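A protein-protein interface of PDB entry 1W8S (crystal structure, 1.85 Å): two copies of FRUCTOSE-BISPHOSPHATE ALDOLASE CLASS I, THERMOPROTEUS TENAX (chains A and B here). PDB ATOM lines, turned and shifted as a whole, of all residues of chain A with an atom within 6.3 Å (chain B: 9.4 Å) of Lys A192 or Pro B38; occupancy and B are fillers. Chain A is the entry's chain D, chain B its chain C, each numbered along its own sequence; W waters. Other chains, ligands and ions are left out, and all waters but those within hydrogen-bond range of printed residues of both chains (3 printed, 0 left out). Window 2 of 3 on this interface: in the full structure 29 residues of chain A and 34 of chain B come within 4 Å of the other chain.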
ATOM      1  N   ARG A 166      23.075 -21.869  -7.179  1.00  0.00           N
ATOM      2  CA  ARG A 166      22.852 -20.546  -6.637  1.00  0.00           C
ATOM      3  C   ARG A 166      23.875 -19.530  -7.169  1.00  0.00           C
ATOM      4  O   ARG A 166      23.524 -18.399  -7.486  1.00  0.00           O
ATOM      5  CB  ARG A 166      22.912 -20.560  -5.121  1.00  0.00           C
ATOM      6  CG  ARG A 166      22.438 -19.267  -4.468  1.00  0.00           C
ATOM      7  CD  ARG A 166      21.102 -18.726  -4.999  1.00  0.00           C
ATOM      8  NE  ARG A 166      20.662 -17.541  -4.252  1.00  0.00           N
ATOM      9  CZ  ARG A 166      19.412 -17.322  -3.865  1.00  0.00           C
ATOM     10  NH1 ARG A 166      18.447 -18.217  -4.121  1.00  0.00           N
ATOM     11  NH2 ARG A 166      19.132 -16.237  -3.172  1.00  0.00           N
ATOM     12  N   LEU A 169      22.932 -18.268 -10.585  1.00  0.00           N
ATOM     13  CA  LEU A 169      21.877 -17.265 -10.511  1.00  0.00           C
ATOM     14  C   LEU A 169      22.468 -15.901 -10.091  1.00  0.00           C
ATOM     15  O   LEU A 169      22.208 -14.875 -10.750  1.00  0.00           O
ATOM     16  CB  LEU A 169      20.783 -17.717  -9.543  1.00  0.00           C
ATOM     17  CG  LEU A 169      19.830 -16.650  -8.995  1.00  0.00           C
ATOM     18  CD1 LEU A 169      19.026 -16.023 -10.082  1.00  0.00           C
ATOM     19  CD2 LEU A 169      18.886 -17.228  -7.938  1.00  0.00           C
ATOM     20  N   PHE A 187      18.067 -32.807  -5.877  1.00  0.00           N
ATOM     21  CA  PHE A 187      18.232 -32.028  -7.082  1.00  0.00           C
ATOM     22  C   PHE A 187      17.153 -30.956  -7.199  1.00  0.00           C
ATOM     23  O   PHE A 187      17.421 -29.882  -7.773  1.00  0.00           O
ATOM     24  CB  PHE A 187      18.258 -32.913  -8.327  1.00  0.00           C
ATOM     25  CG  PHE A 187      18.831 -32.220  -9.538  1.00  0.00           C
ATOM     26  CD1 PHE A 187      20.150 -31.807  -9.545  1.00  0.00           C
ATOM     27  CD2 PHE A 187      18.049 -31.975 -10.669  1.00  0.00           C
ATOM     28  CE1 PHE A 187      20.681 -31.169 -10.659  1.00  0.00           C
ATOM     29  CE2 PHE A 187      18.579 -31.345 -11.784  1.00  0.00           C
ATOM     30  CZ  PHE A 187      19.896 -30.948 -11.781  1.00  0.00           C
ATOM     31  N   SER A 188      15.964 -31.223  -6.630  1.00  0.00           N
ATOM     32  CA  SER A 188      14.865 -30.242  -6.644  1.00  0.00           C
ATOM     33  C   SER A 188      15.178 -29.018  -5.777  1.00  0.00           C
ATOM     34  O   SER A 188      14.688 -27.923  -6.032  1.00  0.00           O
ATOM     35  CB  SER A 188      13.519 -30.868  -6.222  1.00  0.00           C
ATOM     36  OG  SER A 188      13.445 -31.062  -4.829  1.00  0.00           O
ATOM     37  N   TRP A 189      16.004 -29.206  -4.753  1.00  0.00           N
ATOM     38  CA  TRP A 189      16.485 -28.080  -3.955  1.00  0.00           C
ATOM     39  C   TRP A 189      17.447 -27.212  -4.769  1.00  0.00           C
ATOM     40  O   TRP A 189      17.390 -26.012  -4.659  1.00  0.00           O
ATOM     41  CB  TRP A 189      17.148 -28.564  -2.674  1.00  0.00           C
ATOM     42  CG  TRP A 189      17.849 -27.505  -1.876  1.00  0.00           C
ATOM     43  CD1 TRP A 189      19.199 -27.420  -1.644  1.00  0.00           C
ATOM     44  CD2 TRP A 189      17.258 -26.405  -1.169  1.00  0.00           C
ATOM     45  NE1 TRP A 189      19.475 -26.342  -0.838  1.00  0.00           N
ATOM     46  CE2 TRP A 189      18.309 -25.698  -0.535  1.00  0.00           C
ATOM     47  CE3 TRP A 189      15.947 -25.945  -0.999  1.00  0.00           C
ATOM     48  CZ2 TRP A 189      18.094 -24.560   0.223  1.00  0.00           C
ATOM     49  CZ3 TRP A 189      15.736 -24.814  -0.237  1.00  0.00           C
ATOM     50  CH2 TRP A 189      16.798 -24.138   0.370  1.00  0.00           C
ATOM     51  N   ALA A 190      18.316 -27.823  -5.577  1.00  0.00           N
ATOM     52  CA  ALA A 190      19.170 -27.064  -6.481  1.00  0.00           C
ATOM     53  C   ALA A 190      18.299 -26.255  -7.464  1.00  0.00           C
ATOM     54  O   ALA A 190      18.521 -25.033  -7.692  1.00  0.00           O
ATOM     55  CB  ALA A 190      20.153 -28.018  -7.220  1.00  0.00           C
ATOM     56  N   VAL A 191      17.260 -26.897  -7.991  1.00  0.00           N
ATOM     57  CA  VAL A 191      16.365 -26.242  -8.924  1.00  0.00           C
ATOM     58  C   VAL A 191      15.681 -25.036  -8.255  1.00  0.00           C
ATOM     59  O   VAL A 191      15.556 -23.953  -8.871  1.00  0.00           O
ATOM     60  CB  VAL A 191      15.337 -27.222  -9.519  1.00  0.00           C
ATOM     61  CG1 VAL A 191      14.241 -26.468 -10.215  1.00  0.00           C
ATOM     62  CG2 VAL A 191      16.035 -28.185 -10.491  1.00  0.00           C
ATOM     63  N   LYS A 192      15.347 -25.193  -6.986  1.00  0.00           N
ATOM     64  CA  LYS A 192      14.605 -24.195  -6.239  1.00  0.00           C
ATOM     65  C   LYS A 192      15.454 -22.975  -6.052  1.00  0.00           C
ATOM     66  O   LYS A 192      14.993 -21.865  -6.288  1.00  0.00           O
ATOM     67  CB  LYS A 192      14.181 -24.724  -4.846  1.00  0.00           C
ATOM     68  CG  LYS A 192      13.275 -23.760  -4.054  1.00  0.00           C
ATOM     69  CD  LYS A 192      12.842 -24.326  -2.697  1.00  0.00           C
ATOM     70  CE  LYS A 192      11.856 -23.405  -1.954  1.00  0.00           C
ATOM     71  NZ  LYS A 192      11.033 -24.214  -0.980  1.00  0.00           N
ATOM     72  N   VAL A 193      16.680 -23.184  -5.588  1.00  0.00           N
ATOM     73  CA  VAL A 193      17.583 -22.060  -5.300  1.00  0.00           C
ATOM     74  C   VAL A 193      18.041 -21.355  -6.539  1.00  0.00           C
ATOM     75  O   VAL A 193      18.444 -20.192  -6.452  1.00  0.00           O
ATOM     76  CB  VAL A 193      18.782 -22.476  -4.440  1.00  0.00           C
ATOM     77  CG1 VAL A 193      18.259 -23.096  -3.124  1.00  0.00           C
ATOM     78  CG2 VAL A 193      19.693 -23.424  -5.176  1.00  0.00           C
ATOM     79  N   ALA A 194      17.943 -22.022  -7.694  1.00  0.00           N
ATOM     80  CA  ALA A 194      18.177 -21.374  -9.006  1.00  0.00           C
ATOM     81  C   ALA A 194      17.052 -20.361  -9.363  1.00  0.00           C
ATOM     82  O   ALA A 194      17.186 -19.540 -10.280  1.00  0.00           O
ATOM     83  CB  ALA A 194      18.287 -22.431 -10.097  1.00  0.00           C
ATOM     84  N   GLY A 195      15.919 -20.437  -8.665  1.00  0.00           N
ATOM     85  CA  GLY A 195      14.821 -19.499  -8.892  1.00  0.00           C
ATOM     86  C   GLY A 195      14.292 -19.442 -10.319  1.00  0.00           C
ATOM     87  O   GLY A 195      14.021 -20.478 -10.923  1.00  0.00           O
ATOM     88  N   LYS A 196      14.167 -18.223 -10.860  1.00  0.00           N
ATOM     89  CA  LYS A 196      13.688 -17.976 -12.236  1.00  0.00           C
ATOM     90  C   LYS A 196      14.636 -18.456 -13.363  1.00  0.00           C
ATOM     91  O   LYS A 196      14.292 -18.347 -14.530  1.00  0.00           O
ATOM     92  CB  LYS A 196      13.563 -16.463 -12.466  1.00  0.00           C
ATOM     93  CG  LYS A 196      12.454 -15.797 -11.758  1.00  0.00           C
ATOM     94  CD  LYS A 196      12.473 -14.308 -12.131  1.00  0.00           C
ATOM     95  CE  LYS A 196      11.445 -13.547 -11.375  1.00  0.00           C
ATOM     96  NZ  LYS A 196      11.340 -12.178 -11.950  1.00  0.00           N
ATOM     97  N   ALA A 223      12.355 -33.294 -10.703  1.00  0.00           N
ATOM     98  CA  ALA A 223      12.878 -32.244  -9.820  1.00  0.00           C
ATOM     99  C   ALA A 223      12.554 -30.821 -10.323  1.00  0.00           C
ATOM    100  O   ALA A 223      12.782 -29.826  -9.625  1.00  0.00           O
ATOM    101  CB  ALA A 223      14.378 -32.412  -9.661  1.00  0.00           C
ATOM    102  N   TYR B  23      21.603  -9.759   1.555  1.00  0.00           N
ATOM    103  CA  TYR B  23      21.171 -10.971   0.851  1.00  0.00           C
ATOM    104  C   TYR B  23      22.168 -11.329  -0.254  1.00  0.00           C
ATOM    105  O   TYR B  23      21.790 -11.757  -1.337  1.00  0.00           O
ATOM    106  CB  TYR B  23      19.771 -10.771   0.286  1.00  0.00           C
ATOM    107  CG  TYR B  23      19.075 -12.025  -0.181  1.00  0.00           C
ATOM    108  CD1 TYR B  23      18.838 -13.076   0.696  1.00  0.00           C
ATOM    109  CD2 TYR B  23      18.627 -12.154  -1.502  1.00  0.00           C
ATOM    110  CE1 TYR B  23      18.173 -14.224   0.287  1.00  0.00           C
ATOM    111  CE2 TYR B  23      17.957 -13.301  -1.919  1.00  0.00           C
ATOM    112  CZ  TYR B  23      17.731 -14.328  -1.007  1.00  0.00           C
ATOM    113  OH  TYR B  23      17.096 -15.473  -1.403  1.00  0.00           O
ATOM    114  N   PRO B  31      23.548 -21.725  -0.436  1.00  0.00           N
ATOM    115  CA  PRO B  31      22.148 -21.826  -0.035  1.00  0.00           C
ATOM    116  C   PRO B  31      21.891 -22.732   1.169  1.00  0.00           C
ATOM    117  O   PRO B  31      20.737 -22.825   1.560  1.00  0.00           O
ATOM    118  CB  PRO B  31      21.494 -22.355  -1.299  1.00  0.00           C
ATOM    119  CG  PRO B  31      22.505 -23.208  -1.898  1.00  0.00           C
ATOM    120  CD  PRO B  31      23.841 -22.575  -1.596  1.00  0.00           C
ATOM    121  N   ALA B  32      22.917 -23.357   1.761  1.00  0.00           N
ATOM    122  CA  ALA B  32      22.766 -23.986   3.075  1.00  0.00           C
ATOM    123  C   ALA B  32      22.197 -22.989   4.104  1.00  0.00           C
ATOM    124  O   ALA B  32      21.335 -23.360   4.889  1.00  0.00           O
ATOM    125  CB  ALA B  32      24.079 -24.611   3.557  1.00  0.00           C
ATOM    126  N   ASP B  33      22.636 -21.737   4.046  1.00  0.00           N
ATOM    127  CA  ASP B  33      22.047 -20.626   4.822  1.00  0.00           C
ATOM    128  C   ASP B  33      20.494 -20.573   4.759  1.00  0.00           C
ATOM    129  O   ASP B  33      19.887 -20.007   5.659  1.00  0.00           O
ATOM    130  CB  ASP B  33      22.572 -19.257   4.310  1.00  0.00           C
ATOM    131  CG  ASP B  33      23.875 -18.775   5.007  1.00  0.00           C
ATOM    132  OD1 ASP B  33      24.465 -19.522   5.814  1.00  0.00           O
ATOM    133  OD2 ASP B  33      24.369 -17.643   4.806  1.00  0.00           O
ATOM    134  N   PHE B  34      19.880 -21.111   3.694  1.00  0.00           N
ATOM    135  CA  PHE B  34      18.435 -20.968   3.413  1.00  0.00           C
ATOM    136  C   PHE B  34      17.554 -22.128   3.896  1.00  0.00           C
ATOM    137  O   PHE B  34      16.328 -22.034   3.823  1.00  0.00           O
ATOM    138  CB  PHE B  34      18.181 -20.826   1.901  1.00  0.00           C
ATOM    139  CG  PHE B  34      18.943 -19.683   1.227  1.00  0.00           C
ATOM    140  CD1 PHE B  34      19.214 -18.487   1.896  1.00  0.00           C
ATOM    141  CD2 PHE B  34      19.348 -19.796  -0.093  1.00  0.00           C
ATOM    142  CE1 PHE B  34      19.883 -17.438   1.261  1.00  0.00           C
ATOM    143  CE2 PHE B  34      20.016 -18.750  -0.708  1.00  0.00           C
ATOM    144  CZ  PHE B  34      20.301 -17.580  -0.007  1.00  0.00           C
ATOM    145  N   MET B  35      18.152 -23.221   4.363  1.00  0.00           N
ATOM    146  CA  MET B  35      17.373 -24.404   4.726  1.00  0.00           C
ATOM    147  C   MET B  35      16.560 -24.229   6.016  1.00  0.00           C
ATOM    148  O   MET B  35      15.466 -24.767   6.110  1.00  0.00           O
ATOM    149  CB  MET B  35      18.269 -25.652   4.823  1.00  0.00           C
ATOM    150  CG  MET B  35      17.960 -26.719   3.773  1.00  0.00           C
ATOM    151  SD  MET B  35      19.468 -27.581   3.215  1.00  0.00           S
ATOM    152  CE  MET B  35      18.708 -28.862   2.154  1.00  0.00           C
ATOM    153  N   ASP B  36      17.088 -23.476   6.986  1.00  0.00           N
ATOM    154  CA  ASP B  36      16.334 -23.120   8.209  1.00  0.00           C
ATOM    155  C   ASP B  36      14.919 -22.609   7.852  1.00  0.00           C
ATOM    156  O   ASP B  36      13.912 -23.087   8.365  1.00  0.00           O
ATOM    157  CB  ASP B  36      17.081 -22.020   9.007  1.00  0.00           C
ATOM    158  CG  ASP B  36      18.211 -22.570   9.890  1.00  0.00           C
ATOM    159  OD1 ASP B  36      18.524 -23.773   9.780  1.00  0.00           O
ATOM    160  OD2 ASP B  36      18.836 -21.888  10.737  1.00  0.00           O
ATOM    161  N   ASN B  37      14.881 -21.645   6.936  1.00  0.00           N
ATOM    162  CA  ASN B  37      13.672 -20.930   6.517  1.00  0.00           C
ATOM    163  C   ASN B  37      13.627 -20.918   4.971  1.00  0.00           C
ATOM    164  O   ASN B  37      14.076 -19.968   4.353  1.00  0.00           O
ATOM    165  CB  ASN B  37      13.749 -19.506   7.091  1.00  0.00           C
ATOM    166  CG  ASN B  37      12.502 -18.685   6.834  1.00  0.00           C
ATOM    167  OD1 ASN B  37      11.391 -19.208   6.771  1.00  0.00           O
ATOM    168  ND2 ASN B  37      12.682 -17.370   6.719  1.00  0.00           N
ATOM    169  N   PRO B  38      13.160 -21.999   4.346  1.00  0.00           N
ATOM    170  CA  PRO B  38      13.314 -22.172   2.887  1.00  0.00           C
ATOM    171  C   PRO B  38      12.718 -21.041   2.010  1.00  0.00           C
ATOM    172  O   PRO B  38      13.193 -20.852   0.895  1.00  0.00           O
ATOM    173  CB  PRO B  38      12.623 -23.520   2.624  1.00  0.00           C
ATOM    174  CG  PRO B  38      12.707 -24.230   3.937  1.00  0.00           C
ATOM    175  CD  PRO B  38      12.466 -23.149   4.957  1.00  0.00           C
ATOM    176  N   ASP B  39      11.713 -20.301   2.498  1.00  0.00           N
ATOM    177  CA  ASP B  39      11.292 -19.080   1.796  1.00  0.00           C
ATOM    178  C   ASP B  39      12.435 -18.062   1.615  1.00  0.00           C
ATOM    179  O   ASP B  39      12.383 -17.238   0.695  1.00  0.00           O
ATOM    180  CB  ASP B  39      10.140 -18.396   2.515  1.00  0.00           C
ATOM    181  CG  ASP B  39       8.842 -19.168   2.400  1.00  0.00           C
ATOM    182  OD1 ASP B  39       8.820 -20.208   1.702  1.00  0.00           O
ATOM    183  OD2 ASP B  39       7.799 -18.788   2.966  1.00  0.00           O
ATOM    184  N   SER B  40      13.437 -18.088   2.495  1.00  0.00           N
ATOM    185  CA  SER B  40      14.597 -17.189   2.356  1.00  0.00           C
ATOM    186  C   SER B  40      15.408 -17.374   1.073  1.00  0.00           C
ATOM    187  O   SER B  40      16.182 -16.484   0.732  1.00  0.00           O
ATOM    188  CB  SER B  40      15.546 -17.294   3.548  1.00  0.00           C
ATOM    189  OG  SER B  40      16.077 -18.602   3.663  1.00  0.00           O
ATOM    190  N   ALA B  41      15.231 -18.503   0.380  1.00  0.00           N
ATOM    191  CA  ALA B  41      15.853 -18.740  -0.938  1.00  0.00           C
ATOM    192  C   ALA B  41      15.182 -17.968  -2.084  1.00  0.00           C
ATOM    193  O   ALA B  41      15.752 -17.830  -3.177  1.00  0.00           O
ATOM    194  CB  ALA B  41      15.856 -20.231  -1.266  1.00  0.00           C
ATOM    195  N   ASP B  42      13.986 -17.465  -1.813  1.00  0.00           N
ATOM    196  CA  ASP B  42      13.195 -16.686  -2.752  1.00  0.00           C
ATOM    197  C   ASP B  42      13.462 -15.192  -2.542  1.00  0.00           C
ATOM    198  O   ASP B  42      13.088 -14.623  -1.508  1.00  0.00           O
ATOM    199  CB  ASP B  42      11.708 -16.997  -2.523  1.00  0.00           C
ATOM    200  CG  ASP B  42      10.804 -16.363  -3.552  1.00  0.00           C
ATOM    201  OD1 ASP B  42      11.261 -15.549  -4.389  1.00  0.00           O
ATOM    202  OD2 ASP B  42       9.608 -16.647  -3.595  1.00  0.00           O
ATOM    203  N   PRO B  43      14.109 -14.546  -3.496  1.00  0.00           N
ATOM    204  CA  PRO B  43      14.346 -13.102  -3.376  1.00  0.00           C
ATOM    205  C   PRO B  43      13.070 -12.248  -3.300  1.00  0.00           C
ATOM    206  O   PRO B  43      13.127 -11.145  -2.750  1.00  0.00           O
ATOM    207  CB  PRO B  43      15.145 -12.778  -4.647  1.00  0.00           C
ATOM    208  CG  PRO B  43      15.807 -14.090  -5.015  1.00  0.00           C
ATOM    209  CD  PRO B  43      14.721 -15.106  -4.722  1.00  0.00           C
ATOM    210  N   TYR B  45      10.452 -13.013  -1.560  1.00  0.00           N
ATOM    211  CA  TYR B  45      10.192 -13.038  -0.115  1.00  0.00           C
ATOM    212  C   TYR B  45      11.038 -12.024   0.635  1.00  0.00           C
ATOM    213  O   TYR B  45      10.575 -11.343   1.544  1.00  0.00           O
ATOM    214  CB  TYR B  45      10.456 -14.452   0.428  1.00  0.00           C
ATOM    215  CG  TYR B  45      10.551 -14.586   1.934  1.00  0.00           C
ATOM    216  CD1 TYR B  45       9.397 -14.680   2.721  1.00  0.00           C
ATOM    217  CD2 TYR B  45      11.792 -14.668   2.573  1.00  0.00           C
ATOM    218  CE1 TYR B  45       9.479 -14.820   4.114  1.00  0.00           C
ATOM    219  CE2 TYR B  45      11.885 -14.814   3.965  1.00  0.00           C
ATOM    220  CZ  TYR B  45      10.721 -14.885   4.730  1.00  0.00           C
ATOM    221  OH  TYR B  45      10.799 -15.047   6.107  1.00  0.00           O
ATOM    222  N   ILE B  46      12.296 -11.932   0.250  1.00  0.00           N
ATOM    223  CA  ILE B  46      13.241 -11.042   0.913  1.00  0.00           C
ATOM    224  C   ILE B  46      12.826  -9.590   0.728  1.00  0.00           C
ATOM    225  O   ILE B  46      12.920  -8.797   1.636  1.00  0.00           O
ATOM    226  CB  ILE B  46      14.652 -11.293   0.357  1.00  0.00           C
ATOM    227  CG1 ILE B  46      15.109 -12.715   0.683  1.00  0.00           C
ATOM    228  CG2 ILE B  46      15.646 -10.287   0.907  1.00  0.00           C
ATOM    229  CD1 ILE B  46      15.336 -12.996   2.209  1.00  0.00           C
ATOM    230  N   ILE B  64      20.641 -11.441  -8.827  1.00  0.00           N
ATOM    231  CA  ILE B  64      19.386 -11.280  -8.076  1.00  0.00           C
ATOM    232  C   ILE B  64      18.720  -9.928  -8.410  1.00  0.00           C
ATOM    233  O   ILE B  64      17.532  -9.838  -8.592  1.00  0.00           O
ATOM    234  CB  ILE B  64      19.654 -11.377  -6.549  1.00  0.00           C
ATOM    235  CG1 ILE B  64      20.290 -12.736  -6.157  1.00  0.00           C
ATOM    236  CG2 ILE B  64      18.338 -11.211  -5.749  1.00  0.00           C
ATOM    237  CD1 ILE B  64      19.579 -13.965  -6.683  1.00  0.00           C
ATOM    238  N   TYR B  68      15.116 -10.075 -10.173  1.00  0.00           N
ATOM    239  CA  TYR B  68      14.117  -9.889  -9.112  1.00  0.00           C
ATOM    240  C   TYR B  68      13.889  -8.463  -8.644  1.00  0.00           C
ATOM    241  O   TYR B  68      12.846  -8.184  -8.094  1.00  0.00           O
ATOM    242  CB  TYR B  68      14.505 -10.700  -7.888  1.00  0.00           C
ATOM    243  CG  TYR B  68      14.388 -12.184  -8.094  1.00  0.00           C
ATOM    244  CD1 TYR B  68      13.181 -12.845  -7.874  1.00  0.00           C
ATOM    245  CD2 TYR B  68      15.493 -12.933  -8.499  1.00  0.00           C
ATOM    246  CE1 TYR B  68      13.075 -14.227  -8.062  1.00  0.00           C
ATOM    247  CE2 TYR B  68      15.405 -14.306  -8.679  1.00  0.00           C
ATOM    248  CZ  TYR B  68      14.202 -14.946  -8.456  1.00  0.00           C
ATOM    249  OH  TYR B  68      14.102 -16.295  -8.633  1.00  0.00           O
ATOM    250  N   TRP B 235      16.450 -13.297   8.195  1.00  0.00           N
ATOM    251  CA  TRP B 235      15.753 -14.236   7.318  1.00  0.00           C
ATOM    252  C   TRP B 235      16.023 -15.725   7.561  1.00  0.00           C
ATOM    253  O   TRP B 235      15.362 -16.571   6.944  1.00  0.00           O
ATOM    254  CB  TRP B 235      15.906 -13.878   5.829  1.00  0.00           C
ATOM    255  CG  TRP B 235      17.315 -13.588   5.349  1.00  0.00           C
ATOM    256  CD1 TRP B 235      17.805 -12.372   4.977  1.00  0.00           C
ATOM    257  CD2 TRP B 235      18.379 -14.523   5.153  1.00  0.00           C
ATOM    258  NE1 TRP B 235      19.116 -12.484   4.579  1.00  0.00           N
ATOM    259  CE2 TRP B 235      19.498 -13.792   4.675  1.00  0.00           C
ATOM    260  CE3 TRP B 235      18.520 -15.894   5.355  1.00  0.00           C
ATOM    261  CZ2 TRP B 235      20.708 -14.386   4.395  1.00  0.00           C
ATOM    262  CZ3 TRP B 235      19.732 -16.488   5.066  1.00  0.00           C
ATOM    263  CH2 TRP B 235      20.814 -15.739   4.616  1.00  0.00           C
ATOM    264  N   GLN B 236      16.974 -16.041   8.442  1.00  0.00           N
ATOM    265  CA  GLN B 236      17.193 -17.434   8.881  1.00  0.00           C
ATOM    266  C   GLN B 236      16.229 -17.855   9.986  1.00  0.00           C
ATOM    267  O   GLN B 236      16.138 -19.043  10.309  1.00  0.00           O
ATOM    268  CB  GLN B 236      18.648 -17.659   9.368  1.00  0.00           C
ATOM    269  CG  GLN B 236      19.582 -18.292   8.360  1.00  0.00           C
ATOM    270  CD  GLN B 236      20.779 -18.970   9.028  1.00  0.00           C
ATOM    271  OE1 GLN B 236      21.528 -18.332   9.764  1.00  0.00           O
ATOM    272  NE2 GLN B 236      20.910 -20.281   8.820  1.00  0.00           N
ATOM    273  N   ARG B 237      15.529 -16.890  10.578  1.00  0.00           N
ATOM    274  CA  ARG B 237      14.540 -17.168  11.618  1.00  0.00           C
ATOM    275  C   ARG B 237      13.165 -17.516  11.036  1.00  0.00           C
ATOM    276  O   ARG B 237      12.712 -16.922  10.062  1.00  0.00           O
ATOM    277  CB  ARG B 237      14.399 -15.966  12.544  1.00  0.00           C
ATOM    278  CG  ARG B 237      15.704 -15.558  13.181  1.00  0.00           C
ATOM    279  CD  ARG B 237      15.532 -14.566  14.289  1.00  0.00           C
ATOM    280  NE  ARG B 237      16.804 -14.187  14.905  1.00  0.00           N
ATOM    281  CZ  ARG B 237      17.519 -14.971  15.711  1.00  0.00           C
ATOM    282  NH1 ARG B 237      17.120 -16.209  16.010  1.00  0.00           N
ATOM    283  NH2 ARG B 237      18.657 -14.514  16.220  1.00  0.00           N
ATOM    284  N   ARG B 238      12.491 -18.481  11.658  1.00  0.00           N
ATOM    285  CA  ARG B 238      11.148 -18.869  11.217  1.00  0.00           C
ATOM    286  C   ARG B 238      10.065 -17.830  11.611  1.00  0.00           C
ATOM    287  O   ARG B 238       8.974 -17.774  11.007  1.00  0.00           O
ATOM    288  CB  ARG B 238      10.785 -20.245  11.778  1.00  0.00           C
ATOM    289  CG  ARG B 238      10.288 -21.190  10.696  1.00  0.00           C
ATOM    290  CD  ARG B 238      11.374 -22.130  10.163  1.00  0.00           C
ATOM    291  NE  ARG B 238      11.575 -23.240  11.087  1.00  0.00           N
ATOM    292  CZ  ARG B 238      10.690 -24.213  11.299  1.00  0.00           C
ATOM    293  NH1 ARG B 238       9.524 -24.270  10.657  1.00  0.00           N
ATOM    294  NH2 ARG B 238      10.976 -25.152  12.165  1.00  0.00           N
HETATM  295  O   HOH W   1      21.440 -14.569  -1.985  1.00  0.00           O
HETATM  296  O   HOH W   2      14.418 -19.380  -5.263  1.00  0.00           O
HETATM  297  O   HOH W   3      22.270 -26.473   0.389  1.00  0.00           O
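The guanidinium group of Arg A166 sits at hydrogen-bond distance from the backbone carbonyl oxygen of Ala B41 (2.9 Å). OH of Tyr B23 is in hydrogen-bond range of NH2 of Arg A166. The side-chain hydroxyl of Tyr B68 sits at hydrogen-bond distance from the backbone NH of Lys A196.
The backbone carbonyl oxygen of Ser B40 is in hydrogen-bond range of the side-chain hydroxyl of Tyr B23, at 2.5 Å. OH of Tyr B23 lies close to O of Ala B41, 3.2 Å away. The side-chain hydroxyl of Ser B40 lies close to the backbone carbonyl oxygen of Phe B34 (3.4 Å). The backbone carbonyl oxygen of Val A193 lies within hydrogen-bond range of the guanidinium group of Arg A166.
Among the printed residues, pairs that only touch across the chains: Arg A166 with Phe B34, Leu A169 with Ile B64, Trp A189 with Pro B31, Trp A189 with Phe B34, Trp A189 with Met B35, Lys A192 with Pro B38, Val A193 with Pro B31 and Gly A195 with Tyr B68.
Of the printed residues of chain B, Leu A169 touches Ile B64. No residue of chain B comes within 4 Å of Val A191. Of the printed residues of chain B, Lys A192 touches Pro B38 (3.9998 Å). Val A193 touches just one residue of chain B: Pro B31 (3.8 Å). No residue of chain B comes within 4 Å of Ala A194. Printed residues of chain B within 4 Å of Lys A196: Tyr B68 (2.9 Å). Of the printed residues of chain A, Tyr B23 touches Arg A166. Asn B37 touches none of the printed residues of chain A. Printed residues of chain A within 4 Å of Pro B38: Lys A192. Printed residues of chain A within 4 Å of Ala B41: Arg A166 (2.9 Å). Printed residues of chain A within 4 Å of Ile B64: Leu A169. The nearest printed residue of chain A that does not touch Pro B38 is Trp A189 (4.4 Å). The nearest printed residue of chain B that does not touch Trp A189 is Ala B41 (4.3 Å).
Hydrophobic or aromatic side chains of chain A that line the printed part of chain B: Leu A169, Trp A189 and Val A193. Of the 22 printed residues of chain B, 8 touch a printed residue of chain A. Among the printed residues, 11 pairs touch across the chains. Among the printed residues, no Asp or Glu carboxylate lies within 4 Å of a Lys or Arg side-chain nitrogen of the other chain.
No position is printed for both chains.
Water W2 lies within hydrogen-bond range of O of Lys A192 and O of Ala B41. Water W1 lies within hydrogen-bond range of the backbone carbonyl oxygen (O) of Tyr B23 and the guanidinium group (NH2) of Arg A166. Water W3 lies within hydrogen-bond range of NE1 of Trp A189 (3.1 Å) and N of Ala B32 (3.5 Å).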
